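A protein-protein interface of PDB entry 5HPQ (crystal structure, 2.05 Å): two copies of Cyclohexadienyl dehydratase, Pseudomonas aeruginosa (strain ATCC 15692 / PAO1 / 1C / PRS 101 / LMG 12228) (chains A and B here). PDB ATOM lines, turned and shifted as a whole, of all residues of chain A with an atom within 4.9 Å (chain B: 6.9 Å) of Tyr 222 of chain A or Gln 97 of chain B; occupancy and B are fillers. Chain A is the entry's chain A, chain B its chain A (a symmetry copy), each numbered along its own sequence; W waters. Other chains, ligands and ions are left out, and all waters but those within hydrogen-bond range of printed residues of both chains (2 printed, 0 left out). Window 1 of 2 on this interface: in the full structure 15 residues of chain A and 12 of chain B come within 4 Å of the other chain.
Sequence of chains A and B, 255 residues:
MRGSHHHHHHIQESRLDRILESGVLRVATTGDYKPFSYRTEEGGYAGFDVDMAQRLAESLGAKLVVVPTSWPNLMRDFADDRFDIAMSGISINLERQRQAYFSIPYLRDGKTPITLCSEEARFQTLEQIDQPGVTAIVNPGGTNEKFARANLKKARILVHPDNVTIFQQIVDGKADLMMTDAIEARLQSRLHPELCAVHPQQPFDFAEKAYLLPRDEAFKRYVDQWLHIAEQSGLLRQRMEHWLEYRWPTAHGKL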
ATOM      1  N   LEU A  16     -26.926  -6.044 -22.634  1.00  0.00           N
ATOM      2  CA  LEU A  16     -25.736  -5.732 -21.817  1.00  0.00           C
ATOM      3  C   LEU A  16     -24.508  -6.360 -22.484  1.00  0.00           C
ATOM      4  O   LEU A  16     -23.491  -5.729 -22.618  1.00  0.00           O
ATOM      5  CB  LEU A  16     -25.891  -6.296 -20.376  1.00  0.00           C
ATOM      6  CG  LEU A  16     -24.688  -6.279 -19.441  1.00  0.00           C
ATOM      7  CD1 LEU A  16     -24.133  -4.871 -19.321  1.00  0.00           C
ATOM      8  CD2 LEU A  16     -25.059  -6.774 -18.026  1.00  0.00           C
ATOM      9  N   LEU A  56     -22.494   6.472 -17.895  1.00  0.00           N
ATOM     10  CA  LEU A  56     -22.942   5.092 -18.074  1.00  0.00           C
ATOM     11  C   LEU A  56     -22.064   4.433 -19.157  1.00  0.00           C
ATOM     12  O   LEU A  56     -21.652   3.284 -19.027  1.00  0.00           O
ATOM     13  CB  LEU A  56     -24.441   5.016 -18.452  1.00  0.00           C
ATOM     14  CG  LEU A  56     -25.063   3.668 -18.783  1.00  0.00           C
ATOM     15  CD1 LEU A  56     -24.841   2.607 -17.714  1.00  0.00           C
ATOM     16  CD2 LEU A  56     -26.564   3.810 -19.030  1.00  0.00           C
ATOM     17  N   SER A  59     -18.578   3.525 -17.979  1.00  0.00           N
ATOM     18  CA  SER A  59     -18.561   2.440 -16.997  1.00  0.00           C
ATOM     19  C   SER A  59     -18.559   1.149 -17.748  1.00  0.00           C
ATOM     20  O   SER A  59     -18.102   0.169 -17.243  1.00  0.00           O
ATOM     21  CB  SER A  59     -19.801   2.510 -16.034  1.00  0.00           C
ATOM     22  OG  SER A  59     -20.931   1.894 -16.612  1.00  0.00           O
ATOM     23  N   LEU A  60     -19.127   1.153 -18.946  1.00  0.00           N
ATOM     24  CA  LEU A  60     -19.218  -0.016 -19.811  1.00  0.00           C
ATOM     25  C   LEU A  60     -18.058  -0.137 -20.819  1.00  0.00           C
ATOM     26  O   LEU A  60     -18.064  -1.018 -21.624  1.00  0.00           O
ATOM     27  CB  LEU A  60     -20.558  -0.008 -20.561  1.00  0.00           C
ATOM     28  CG  LEU A  60     -21.826  -0.265 -19.760  1.00  0.00           C
ATOM     29  CD1 LEU A  60     -23.113   0.116 -20.486  1.00  0.00           C
ATOM     30  CD2 LEU A  60     -21.885  -1.669 -19.269  1.00  0.00           C
ATOM     31  N   ALA A 218     -31.044  -8.285 -17.476  1.00  0.00           N
ATOM     32  CA  ALA A 218     -29.654  -8.087 -17.096  1.00  0.00           C
ATOM     33  C   ALA A 218     -29.235  -6.644 -17.314  1.00  0.00           C
ATOM     34  O   ALA A 218     -28.558  -6.075 -16.478  1.00  0.00           O
ATOM     35  CB  ALA A 218     -28.739  -9.027 -17.842  1.00  0.00           C
ATOM     36  N   PHE A 219     -29.620  -6.058 -18.425  1.00  0.00           N
ATOM     37  CA  PHE A 219     -29.265  -4.620 -18.672  1.00  0.00           C
ATOM     38  C   PHE A 219     -29.934  -3.658 -17.690  1.00  0.00           C
ATOM     39  O   PHE A 219     -29.263  -2.759 -17.165  1.00  0.00           O
ATOM     40  CB  PHE A 219     -29.538  -4.205 -20.113  1.00  0.00           C
ATOM     41  CG  PHE A 219     -28.977  -2.863 -20.488  1.00  0.00           C
ATOM     42  CD1 PHE A 219     -27.645  -2.545 -20.258  1.00  0.00           C
ATOM     43  CD2 PHE A 219     -29.776  -1.949 -21.095  1.00  0.00           C
ATOM     44  CE1 PHE A 219     -27.131  -1.333 -20.650  1.00  0.00           C
ATOM     45  CE2 PHE A 219     -29.309  -0.688 -21.434  1.00  0.00           C
ATOM     46  CZ  PHE A 219     -27.996  -0.365 -21.203  1.00  0.00           C
ATOM     47  N   LYS A 220     -31.216  -3.862 -17.352  1.00  0.00           N
ATOM     48  CA  LYS A 220     -31.795  -3.058 -16.239  1.00  0.00           C
ATOM     49  C   LYS A 220     -31.036  -3.176 -14.946  1.00  0.00           C
ATOM     50  O   LYS A 220     -30.834  -2.181 -14.254  1.00  0.00           O
ATOM     51  CB  LYS A 220     -33.226  -3.430 -15.931  1.00  0.00           C
ATOM     52  CG  LYS A 220     -33.824  -2.627 -14.784  1.00  0.00           C
ATOM     53  CD  LYS A 220     -35.310  -2.911 -14.640  1.00  0.00           C
ATOM     54  CE  LYS A 220     -35.945  -2.568 -13.289  1.00  0.00           C
ATOM     55  NZ  LYS A 220     -35.668  -1.149 -12.872  1.00  0.00           N
ATOM     56  N   ARG A 221     -30.628  -4.400 -14.591  1.00  0.00           N
ATOM     57  CA  ARG A 221     -29.882  -4.625 -13.369  1.00  0.00           C
ATOM     58  C   ARG A 221     -28.604  -3.854 -13.355  1.00  0.00           C
ATOM     59  O   ARG A 221     -28.189  -3.303 -12.305  1.00  0.00           O
ATOM     60  CB  ARG A 221     -29.536  -6.117 -13.179  1.00  0.00           C
ATOM     61  CG  ARG A 221     -30.415  -6.932 -12.278  1.00  0.00           C
ATOM     62  CD  ARG A 221     -31.847  -6.607 -12.473  1.00  0.00           C
ATOM     63  NE  ARG A 221     -32.713  -7.639 -11.881  1.00  0.00           N
ATOM     64  CZ  ARG A 221     -33.533  -7.432 -10.878  1.00  0.00           C
ATOM     65  NH1 ARG A 221     -33.594  -6.261 -10.260  1.00  0.00           N
ATOM     66  NH2 ARG A 221     -34.308  -8.412 -10.474  1.00  0.00           N
ATOM     67  N   TYR A 222     -27.892  -3.880 -14.479  1.00  0.00           N
ATOM     68  CA  TYR A 222     -26.594  -3.128 -14.592  1.00  0.00           C
ATOM     69  C   TYR A 222     -26.862  -1.648 -14.437  1.00  0.00           C
ATOM     70  O   TYR A 222     -26.193  -0.961 -13.662  1.00  0.00           O
ATOM     71  CB  TYR A 222     -25.873  -3.380 -15.914  1.00  0.00           C
ATOM     72  CG  TYR A 222     -24.587  -2.637 -15.972  1.00  0.00           C
ATOM     73  CD1 TYR A 222     -24.539  -1.298 -16.353  1.00  0.00           C
ATOM     74  CD2 TYR A 222     -23.394  -3.252 -15.602  1.00  0.00           C
ATOM     75  CE1 TYR A 222     -23.344  -0.617 -16.356  1.00  0.00           C
ATOM     76  CE2 TYR A 222     -22.189  -2.591 -15.661  1.00  0.00           C
ATOM     77  CZ  TYR A 222     -22.152  -1.292 -16.026  1.00  0.00           C
ATOM     78  OH  TYR A 222     -20.939  -0.644 -15.992  1.00  0.00           O
ATOM     79  N   VAL A 223     -27.859  -1.144 -15.153  1.00  0.00           N
ATOM     80  CA  VAL A 223     -28.167   0.286 -15.116  1.00  0.00           C
ATOM     81  C   VAL A 223     -28.551   0.748 -13.703  1.00  0.00           C
ATOM     82  O   VAL A 223     -28.021   1.745 -13.183  1.00  0.00           O
ATOM     83  CB  VAL A 223     -29.275   0.637 -16.140  1.00  0.00           C
ATOM     84  CG1 VAL A 223     -29.724   2.078 -16.013  1.00  0.00           C
ATOM     85  CG2 VAL A 223     -28.750   0.438 -17.572  1.00  0.00           C
ATOM     86  N   ASP A 224     -29.440   0.003 -13.079  1.00  0.00           N
ATOM     87  CA  ASP A 224     -29.854   0.298 -11.715  1.00  0.00           C
ATOM     88  C   ASP A 224     -28.683   0.217 -10.751  1.00  0.00           C
ATOM     89  O   ASP A 224     -28.593   1.021  -9.869  1.00  0.00           O
ATOM     90  CB  ASP A 224     -30.903  -0.693 -11.238  1.00  0.00           C
ATOM     91  CG  ASP A 224     -32.263  -0.495 -11.922  1.00  0.00           C
ATOM     92  OD1 ASP A 224     -32.478   0.599 -12.570  1.00  0.00           O
ATOM     93  OD2 ASP A 224     -33.133  -1.409 -11.738  1.00  0.00           O
ATOM     94  N   GLN A 225     -27.828  -0.790 -10.889  1.00  0.00           N
ATOM     95  CA  GLN A 225     -26.669  -0.834 -10.021  1.00  0.00           C
ATOM     96  C   GLN A 225     -25.784   0.425 -10.184  1.00  0.00           C
ATOM     97  O   GLN A 225     -25.343   1.007  -9.163  1.00  0.00           O
ATOM     98  CB  GLN A 225     -25.836  -2.095 -10.217  1.00  0.00           C
ATOM     99  CG  GLN A 225     -25.002  -2.458  -9.018  1.00  0.00           C
ATOM    100  CD  GLN A 225     -25.875  -2.877  -7.853  1.00  0.00           C
ATOM    101  OE1 GLN A 225     -26.037  -2.149  -6.921  1.00  0.00           O
ATOM    102  NE2 GLN A 225     -26.363  -4.080  -7.881  1.00  0.00           N
ATOM    103  N   TRP A 226     -25.560   0.837 -11.430  1.00  0.00           N
ATOM    104  CA  TRP A 226     -24.748   2.016 -11.718  1.00  0.00           C
ATOM    105  C   TRP A 226     -25.414   3.276 -11.127  1.00  0.00           C
ATOM    106  O   TRP A 226     -24.739   4.160 -10.568  1.00  0.00           O
ATOM    107  CB  TRP A 226     -24.547   2.154 -13.213  1.00  0.00           C
ATOM    108  CG  TRP A 226     -24.184   3.539 -13.680  1.00  0.00           C
ATOM    109  CD1 TRP A 226     -22.973   4.119 -13.629  1.00  0.00           C
ATOM    110  CD2 TRP A 226     -25.084   4.534 -14.234  1.00  0.00           C
ATOM    111  NE1 TRP A 226     -23.051   5.401 -14.112  1.00  0.00           N
ATOM    112  CE2 TRP A 226     -24.325   5.672 -14.505  1.00  0.00           C
ATOM    113  CE3 TRP A 226     -26.449   4.555 -14.527  1.00  0.00           C
ATOM    114  CZ2 TRP A 226     -24.889   6.824 -15.044  1.00  0.00           C
ATOM    115  CZ3 TRP A 226     -26.995   5.666 -15.074  1.00  0.00           C
ATOM    116  CH2 TRP A 226     -26.231   6.776 -15.347  1.00  0.00           C
ATOM    117  N   MET B  75     -14.536 -14.826 -10.532  1.00  0.00           N
ATOM    118  CA  MET B  75     -15.387 -14.616 -11.722  1.00  0.00           C
ATOM    119  C   MET B  75     -15.238 -15.778 -12.755  1.00  0.00           C
ATOM    120  O   MET B  75     -16.224 -16.262 -13.301  1.00  0.00           O
ATOM    121  CB  MET B  75     -15.137 -13.197 -12.304  1.00  0.00           C
ATOM    122  CG  MET B  75     -15.532 -12.085 -11.311  1.00  0.00           C
ATOM    123  SD  MET B  75     -17.177 -12.249 -10.562  1.00  0.00           S
ATOM    124  CE  MET B  75     -18.232 -12.397 -11.991  1.00  0.00           C
ATOM    125  N   ILE B  92     -20.242  -5.113  -4.070  1.00  0.00           N
ATOM    126  CA  ILE B  92     -20.822  -4.827  -5.333  1.00  0.00           C
ATOM    127  C   ILE B  92     -19.877  -3.965  -6.174  1.00  0.00           C
ATOM    128  O   ILE B  92     -19.378  -2.985  -5.683  1.00  0.00           O
ATOM    129  CB  ILE B  92     -22.160  -4.067  -5.160  1.00  0.00           C
ATOM    130  CG1 ILE B  92     -23.233  -5.061  -4.623  1.00  0.00           C
ATOM    131  CG2 ILE B  92     -22.615  -3.498  -6.502  1.00  0.00           C
ATOM    132  CD1 ILE B  92     -24.677  -4.544  -4.499  1.00  0.00           C
ATOM    133  N   ASN B  93     -19.597  -4.320  -7.435  1.00  0.00           N
ATOM    134  CA  ASN B  93     -19.024  -3.296  -8.328  1.00  0.00           C
ATOM    135  C   ASN B  93     -19.490  -3.548  -9.717  1.00  0.00           C
ATOM    136  O   ASN B  93     -19.992  -4.656  -9.985  1.00  0.00           O
ATOM    137  CB  ASN B  93     -17.486  -3.116  -8.210  1.00  0.00           C
ATOM    138  CG  ASN B  93     -16.693  -4.283  -8.770  1.00  0.00           C
ATOM    139  OD1 ASN B  93     -17.240  -5.216  -9.343  1.00  0.00           O
ATOM    140  ND2 ASN B  93     -15.373  -4.211  -8.619  1.00  0.00           N
ATOM    141  N   LEU B  94     -19.350  -2.560 -10.597  1.00  0.00           N
ATOM    142  CA  LEU B  94     -19.886  -2.738 -11.973  1.00  0.00           C
ATOM    143  C   LEU B  94     -19.141  -3.732 -12.820  1.00  0.00           C
ATOM    144  O   LEU B  94     -19.744  -4.441 -13.623  1.00  0.00           O
ATOM    145  CB  LEU B  94     -20.059  -1.406 -12.695  1.00  0.00           C
ATOM    146  CG  LEU B  94     -21.019  -0.498 -11.916  1.00  0.00           C
ATOM    147  CD1 LEU B  94     -20.981   0.889 -12.563  1.00  0.00           C
ATOM    148  CD2 LEU B  94     -22.426  -1.083 -11.833  1.00  0.00           C
ATOM    149  N   GLU B  95     -17.836  -3.857 -12.617  1.00  0.00           N
ATOM    150  CA  GLU B  95     -17.088  -4.912 -13.338  1.00  0.00           C
ATOM    151  C   GLU B  95     -17.740  -6.273 -13.119  1.00  0.00           C
ATOM    152  O   GLU B  95     -17.921  -7.061 -14.050  1.00  0.00           O
ATOM    153  CB  GLU B  95     -15.621  -4.942 -12.870  1.00  0.00           C
ATOM    154  CG  GLU B  95     -14.710  -6.010 -13.490  1.00  0.00           C
ATOM    155  CD  GLU B  95     -13.212  -5.776 -13.131  1.00  0.00           C
ATOM    156  OE1 GLU B  95     -12.701  -4.675 -13.337  1.00  0.00           O
ATOM    157  OE2 GLU B  95     -12.540  -6.690 -12.612  1.00  0.00           O
ATOM    158  N   ARG B  96     -18.074  -6.554 -11.861  1.00  0.00           N
ATOM    159  CA  ARG B  96     -18.677  -7.830 -11.491  1.00  0.00           C
ATOM    160  C   ARG B  96     -20.101  -7.899 -12.050  1.00  0.00           C
ATOM    161  O   ARG B  96     -20.550  -8.972 -12.556  1.00  0.00           O
ATOM    162  CB  ARG B  96     -18.674  -8.027  -9.981  1.00  0.00           C
ATOM    163  CG  ARG B  96     -17.400  -8.660  -9.498  1.00  0.00           C
ATOM    164  CD  ARG B  96     -17.175  -8.394  -8.018  1.00  0.00           C
ATOM    165  NE  ARG B  96     -15.822  -8.774  -7.621  1.00  0.00           N
ATOM    166  CZ  ARG B  96     -15.314  -8.506  -6.421  1.00  0.00           C
ATOM    167  NH1 ARG B  96     -16.090  -7.898  -5.501  1.00  0.00           N
ATOM    168  NH2 ARG B  96     -14.057  -8.908  -6.117  1.00  0.00           N
ATOM    169  N   GLN B  97     -20.767  -6.728 -12.040  1.00  0.00           N
ATOM    170  CA  GLN B  97     -22.132  -6.674 -12.538  1.00  0.00           C
ATOM    171  C   GLN B  97     -22.209  -6.959 -14.010  1.00  0.00           C
ATOM    172  O   GLN B  97     -23.278  -7.274 -14.496  1.00  0.00           O
ATOM    173  CB  GLN B  97     -22.720  -5.303 -12.258  1.00  0.00           C
ATOM    174  CG  GLN B  97     -24.229  -5.173 -12.484  1.00  0.00           C
ATOM    175  CD  GLN B  97     -25.119  -5.794 -11.401  1.00  0.00           C
ATOM    176  OE1 GLN B  97     -24.914  -5.589 -10.209  1.00  0.00           O
ATOM    177  NE2 GLN B  97     -26.145  -6.532 -11.821  1.00  0.00           N
ATOM    178  N   ARG B  98     -21.098  -6.771 -14.753  1.00  0.00           N
ATOM    179  CA  ARG B  98     -21.043  -7.111 -16.183  1.00  0.00           C
ATOM    180  C   ARG B  98     -21.435  -8.532 -16.531  1.00  0.00           C
ATOM    181  O   ARG B  98     -22.102  -8.777 -17.583  1.00  0.00           O
ATOM    182  CB  ARG B  98     -19.642  -6.799 -16.804  1.00  0.00           C
ATOM    183  CG  ARG B  98     -19.273  -5.343 -16.814  1.00  0.00           C
ATOM    184  CD  ARG B  98     -17.925  -5.118 -17.504  1.00  0.00           C
ATOM    185  NE  ARG B  98     -17.572  -3.703 -17.564  1.00  0.00           N
ATOM    186  CZ  ARG B  98     -16.607  -3.188 -18.348  1.00  0.00           C
ATOM    187  NH1 ARG B  98     -15.940  -3.959 -19.209  1.00  0.00           N
ATOM    188  NH2 ARG B  98     -16.349  -1.889 -18.328  1.00  0.00           N
ATOM    189  N   GLN B  99     -21.058  -9.455 -15.648  1.00  0.00           N
ATOM    190  CA  GLN B  99     -21.262 -10.860 -15.855  1.00  0.00           C
ATOM    191  C   GLN B  99     -22.304 -11.451 -14.900  1.00  0.00           C
ATOM    192  O   GLN B  99     -23.028 -12.330 -15.266  1.00  0.00           O
ATOM    193  CB  GLN B  99     -19.981 -11.619 -15.555  1.00  0.00           C
ATOM    194  CG  GLN B  99     -18.730 -11.339 -16.389  1.00  0.00           C
ATOM    195  CD  GLN B  99     -17.567 -12.170 -15.845  1.00  0.00           C
ATOM    196  OE1 GLN B  99     -16.601 -11.627 -15.277  1.00  0.00           O
ATOM    197  NE2 GLN B  99     -17.703 -13.505 -15.914  1.00  0.00           N
ATOM    198  N   ALA B 100     -22.325 -11.006 -13.649  1.00  0.00           N
ATOM    199  CA  ALA B 100     -23.219 -11.625 -12.643  1.00  0.00           C
ATOM    200  C   ALA B 100     -24.374 -10.656 -12.186  1.00  0.00           C
ATOM    201  O   ALA B 100     -24.442  -9.483 -12.593  1.00  0.00           O
ATOM    202  CB  ALA B 100     -22.382 -11.987 -11.427  1.00  0.00           C
ATOM    203  N   TYR B 101     -25.214 -11.186 -11.299  1.00  0.00           N
ATOM    204  CA  TYR B 101     -26.169 -10.426 -10.499  1.00  0.00           C
ATOM    205  C   TYR B 101     -25.674 -10.321  -9.072  1.00  0.00           C
ATOM    206  O   TYR B 101     -24.949 -11.179  -8.579  1.00  0.00           O
ATOM    207  CB  TYR B 101     -27.543 -11.075 -10.423  1.00  0.00           C
ATOM    208  CG  TYR B 101     -28.467 -10.965 -11.619  1.00  0.00           C
ATOM    209  CD1 TYR B 101     -28.160 -10.132 -12.687  1.00  0.00           C
ATOM    210  CD2 TYR B 101     -29.687 -11.680 -11.681  1.00  0.00           C
ATOM    211  CE1 TYR B 101     -28.985 -10.028 -13.758  1.00  0.00           C
ATOM    212  CE2 TYR B 101     -30.583 -11.473 -12.777  1.00  0.00           C
ATOM    213  CZ  TYR B 101     -30.156 -10.679 -13.809  1.00  0.00           C
ATOM    214  OH  TYR B 101     -30.857 -10.435 -14.964  1.00  0.00           O
ATOM    215  N   PHE B 102     -26.137  -9.295  -8.372  1.00  0.00           N
ATOM    216  CA  PHE B 102     -26.021  -9.266  -6.936  1.00  0.00           C
ATOM    217  C   PHE B 102     -27.396  -9.321  -6.318  1.00  0.00           C
ATOM    218  O   PHE B 102     -28.345  -8.681  -6.826  1.00  0.00           O
ATOM    219  CB  PHE B 102     -25.336  -7.968  -6.465  1.00  0.00           C
ATOM    220  CG  PHE B 102     -23.894  -7.924  -6.781  1.00  0.00           C
ATOM    221  CD1 PHE B 102     -22.991  -8.558  -5.965  1.00  0.00           C
ATOM    222  CD2 PHE B 102     -23.436  -7.313  -7.933  1.00  0.00           C
ATOM    223  CE1 PHE B 102     -21.626  -8.532  -6.247  1.00  0.00           C
ATOM    224  CE2 PHE B 102     -22.078  -7.299  -8.230  1.00  0.00           C
ATOM    225  CZ  PHE B 102     -21.191  -7.912  -7.406  1.00  0.00           C
ATOM    226  N   LEU B 212     -23.234 -12.815  -4.597  1.00  0.00           N
ATOM    227  CA  LEU B 212     -22.995 -12.907  -6.030  1.00  0.00           C
ATOM    228  C   LEU B 212     -23.896 -14.022  -6.555  1.00  0.00           C
ATOM    229  O   LEU B 212     -23.860 -15.127  -6.051  1.00  0.00           O
ATOM    230  CB  LEU B 212     -21.537 -13.229  -6.351  1.00  0.00           C
ATOM    231  CG  LEU B 212     -21.137 -13.084  -7.825  1.00  0.00           C
ATOM    232  CD1 LEU B 212     -20.883 -11.623  -8.156  1.00  0.00           C
ATOM    233  CD2 LEU B 212     -19.897 -13.845  -8.232  1.00  0.00           C
ATOM    234  N   ARG B 215     -27.202 -14.824 -13.468  1.00  0.00           N
ATOM    235  CA  ARG B 215     -28.270 -14.120 -14.147  1.00  0.00           C
ATOM    236  C   ARG B 215     -29.482 -15.058 -14.181  1.00  0.00           C
ATOM    237  O   ARG B 215     -29.746 -15.711 -15.171  1.00  0.00           O
ATOM    238  CB  ARG B 215     -27.879 -13.729 -15.572  1.00  0.00           C
ATOM    239  CG  ARG B 215     -26.709 -12.787 -15.716  1.00  0.00           C
ATOM    240  CD  ARG B 215     -26.666 -12.330 -17.159  1.00  0.00           C
ATOM    241  NE  ARG B 215     -25.568 -11.405 -17.394  1.00  0.00           N
ATOM    242  CZ  ARG B 215     -25.201 -10.985 -18.614  1.00  0.00           C
ATOM    243  NH1 ARG B 215     -25.797 -11.447 -19.649  1.00  0.00           N
ATOM    244  NH2 ARG B 215     -24.203 -10.144 -18.788  1.00  0.00           N
HETATM  245  O   HOH W   1     -18.599  -2.227 -15.366  1.00  0.00           O
HETATM  246  O   HOH W   2     -26.613  -7.082 -14.619  1.00  0.00           O
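O of Ser 59 of chain A is in hydrogen-bond range of NH2 of Arg 98 of chain B (2.9 Å). The side-chain hydroxyl of Tyr 101 of chain B sits at hydrogen-bond distance from the backbone NH of Ala 218 of chain A, at 3.3 Å. The side-chain amide nitrogen (NE2) of Gln 225 of chain A is in hydrogen-bond range of the side-chain amide oxygen (OE1) of Gln 97 of chain B (3.1 Å).
The side-chain hydroxyl (OG) of Ser 59 of chain A lies within hydrogen-bond range of the backbone carbonyl oxygen (O) of Leu 56 of chain A, at 2.9 Å. OG of Ser 59 of chain A lies within hydrogen-bond range of OH of Tyr 222 of chain A, at 2.6 Å. The side-chain amide nitrogen of Gln 97 of chain B lies within hydrogen-bond range of the backbone carbonyl oxygen of Ala 100 of chain B, at 3.5 Å. O of Arg 98 of chain B is in hydrogen-bond range of NH2 of Arg 215 of chain B (2.8 Å). The backbone carbonyl oxygen (O) of Gln 99 of chain B is in hydrogen-bond range of the guanidinium group (NE) of Arg 215 of chain B, 3.4 Å away.
Among the printed residues, pairs that only touch across the chains: Leu 60 of chain A with Arg 98 of chain B (3.5 Å), Tyr 222 of chain A with Leu 94 of chain B (3.5 Å), Leu 16 of chain A with Arg 215 of chain B (3.6 Å), Gln 225 of chain A with Ile 92 of chain B (3.6 Å), Leu 16 of chain A with Arg 98 of chain B (3.6 Å), Arg 221 of chain A with Gln 97 of chain B (3.7 Å), Trp 226 of chain A with Leu 94 of chain B (3.7 Å), Arg 221 of chain A with Tyr 101 of chain B (3.7 Å), Tyr 222 of chain A with Gln 97 of chain B (3.8 Å), Gln 225 of chain A with Leu 94 of chain B (3.9 Å), Ala 218 of chain A with Arg 215 of chain B (3.96 Å) and Leu 16 of chain A with Gln 97 of chain B (3.99 Å).
Of the printed residues of chain B, Ser 59 of chain A touches Arg 98. Of the printed residues of chain B, Ala 218 of chain A touches Tyr 101 and Arg 215. Of the printed residues of chain B, Arg 221 of chain A touches Gln 97 (3.7 Å) and Tyr 101 (3.7 Å). Tyr 222 of chain A touches just these residues of chain B: Leu 94 and Gln 97. Printed residues of chain B within 4 Å of Gln 225 of chain A: Ile 92, Leu 94 and Gln 97. Printed residues of chain A within 4 Å of Gln 97 of chain B: Leu 16, Arg 221, Tyr 222 and Gln 225. Printed residues of chain A within 4 Å of Tyr 101 of chain B: Ala 218 (3.3 Å) and Arg 221 (3.7 Å). The nearest residue of chain B that does not touch Tyr 222 of chain A is Arg 98 of chain B (4.2 Å).
Along chain B the printed residues that touch a printed residue of chain A span positions 92 to 215. Among the printed residues, no Asp or Glu carboxylate lies within 4 Å of a Lys or Arg side-chain nitrogen of the other chain.
No position is printed for both chains. Of the 15 pairs that touch across the chains among the printed residues, none has its exchanged pair printed and touching as well.
Water W1 lies within hydrogen-bond range of NE of Arg 98 of chain B (2.8 Å), OH of Tyr 222 of chain A (2.9 Å), O of Leu 94 of chain B (3.0 Å), O of Ser 59 of chain A (3.1 Å) and N of Glu 95 of chain B (3.3 Å). Water W2 lies within hydrogen-bond range of the backbone carbonyl oxygen of Ala 218 of chain A (2.9 Å), the side-chain amide nitrogen of Gln 97 of chain B (2.9 Å) and the backbone NH of Tyr 222 of chain A (3.5 Å).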
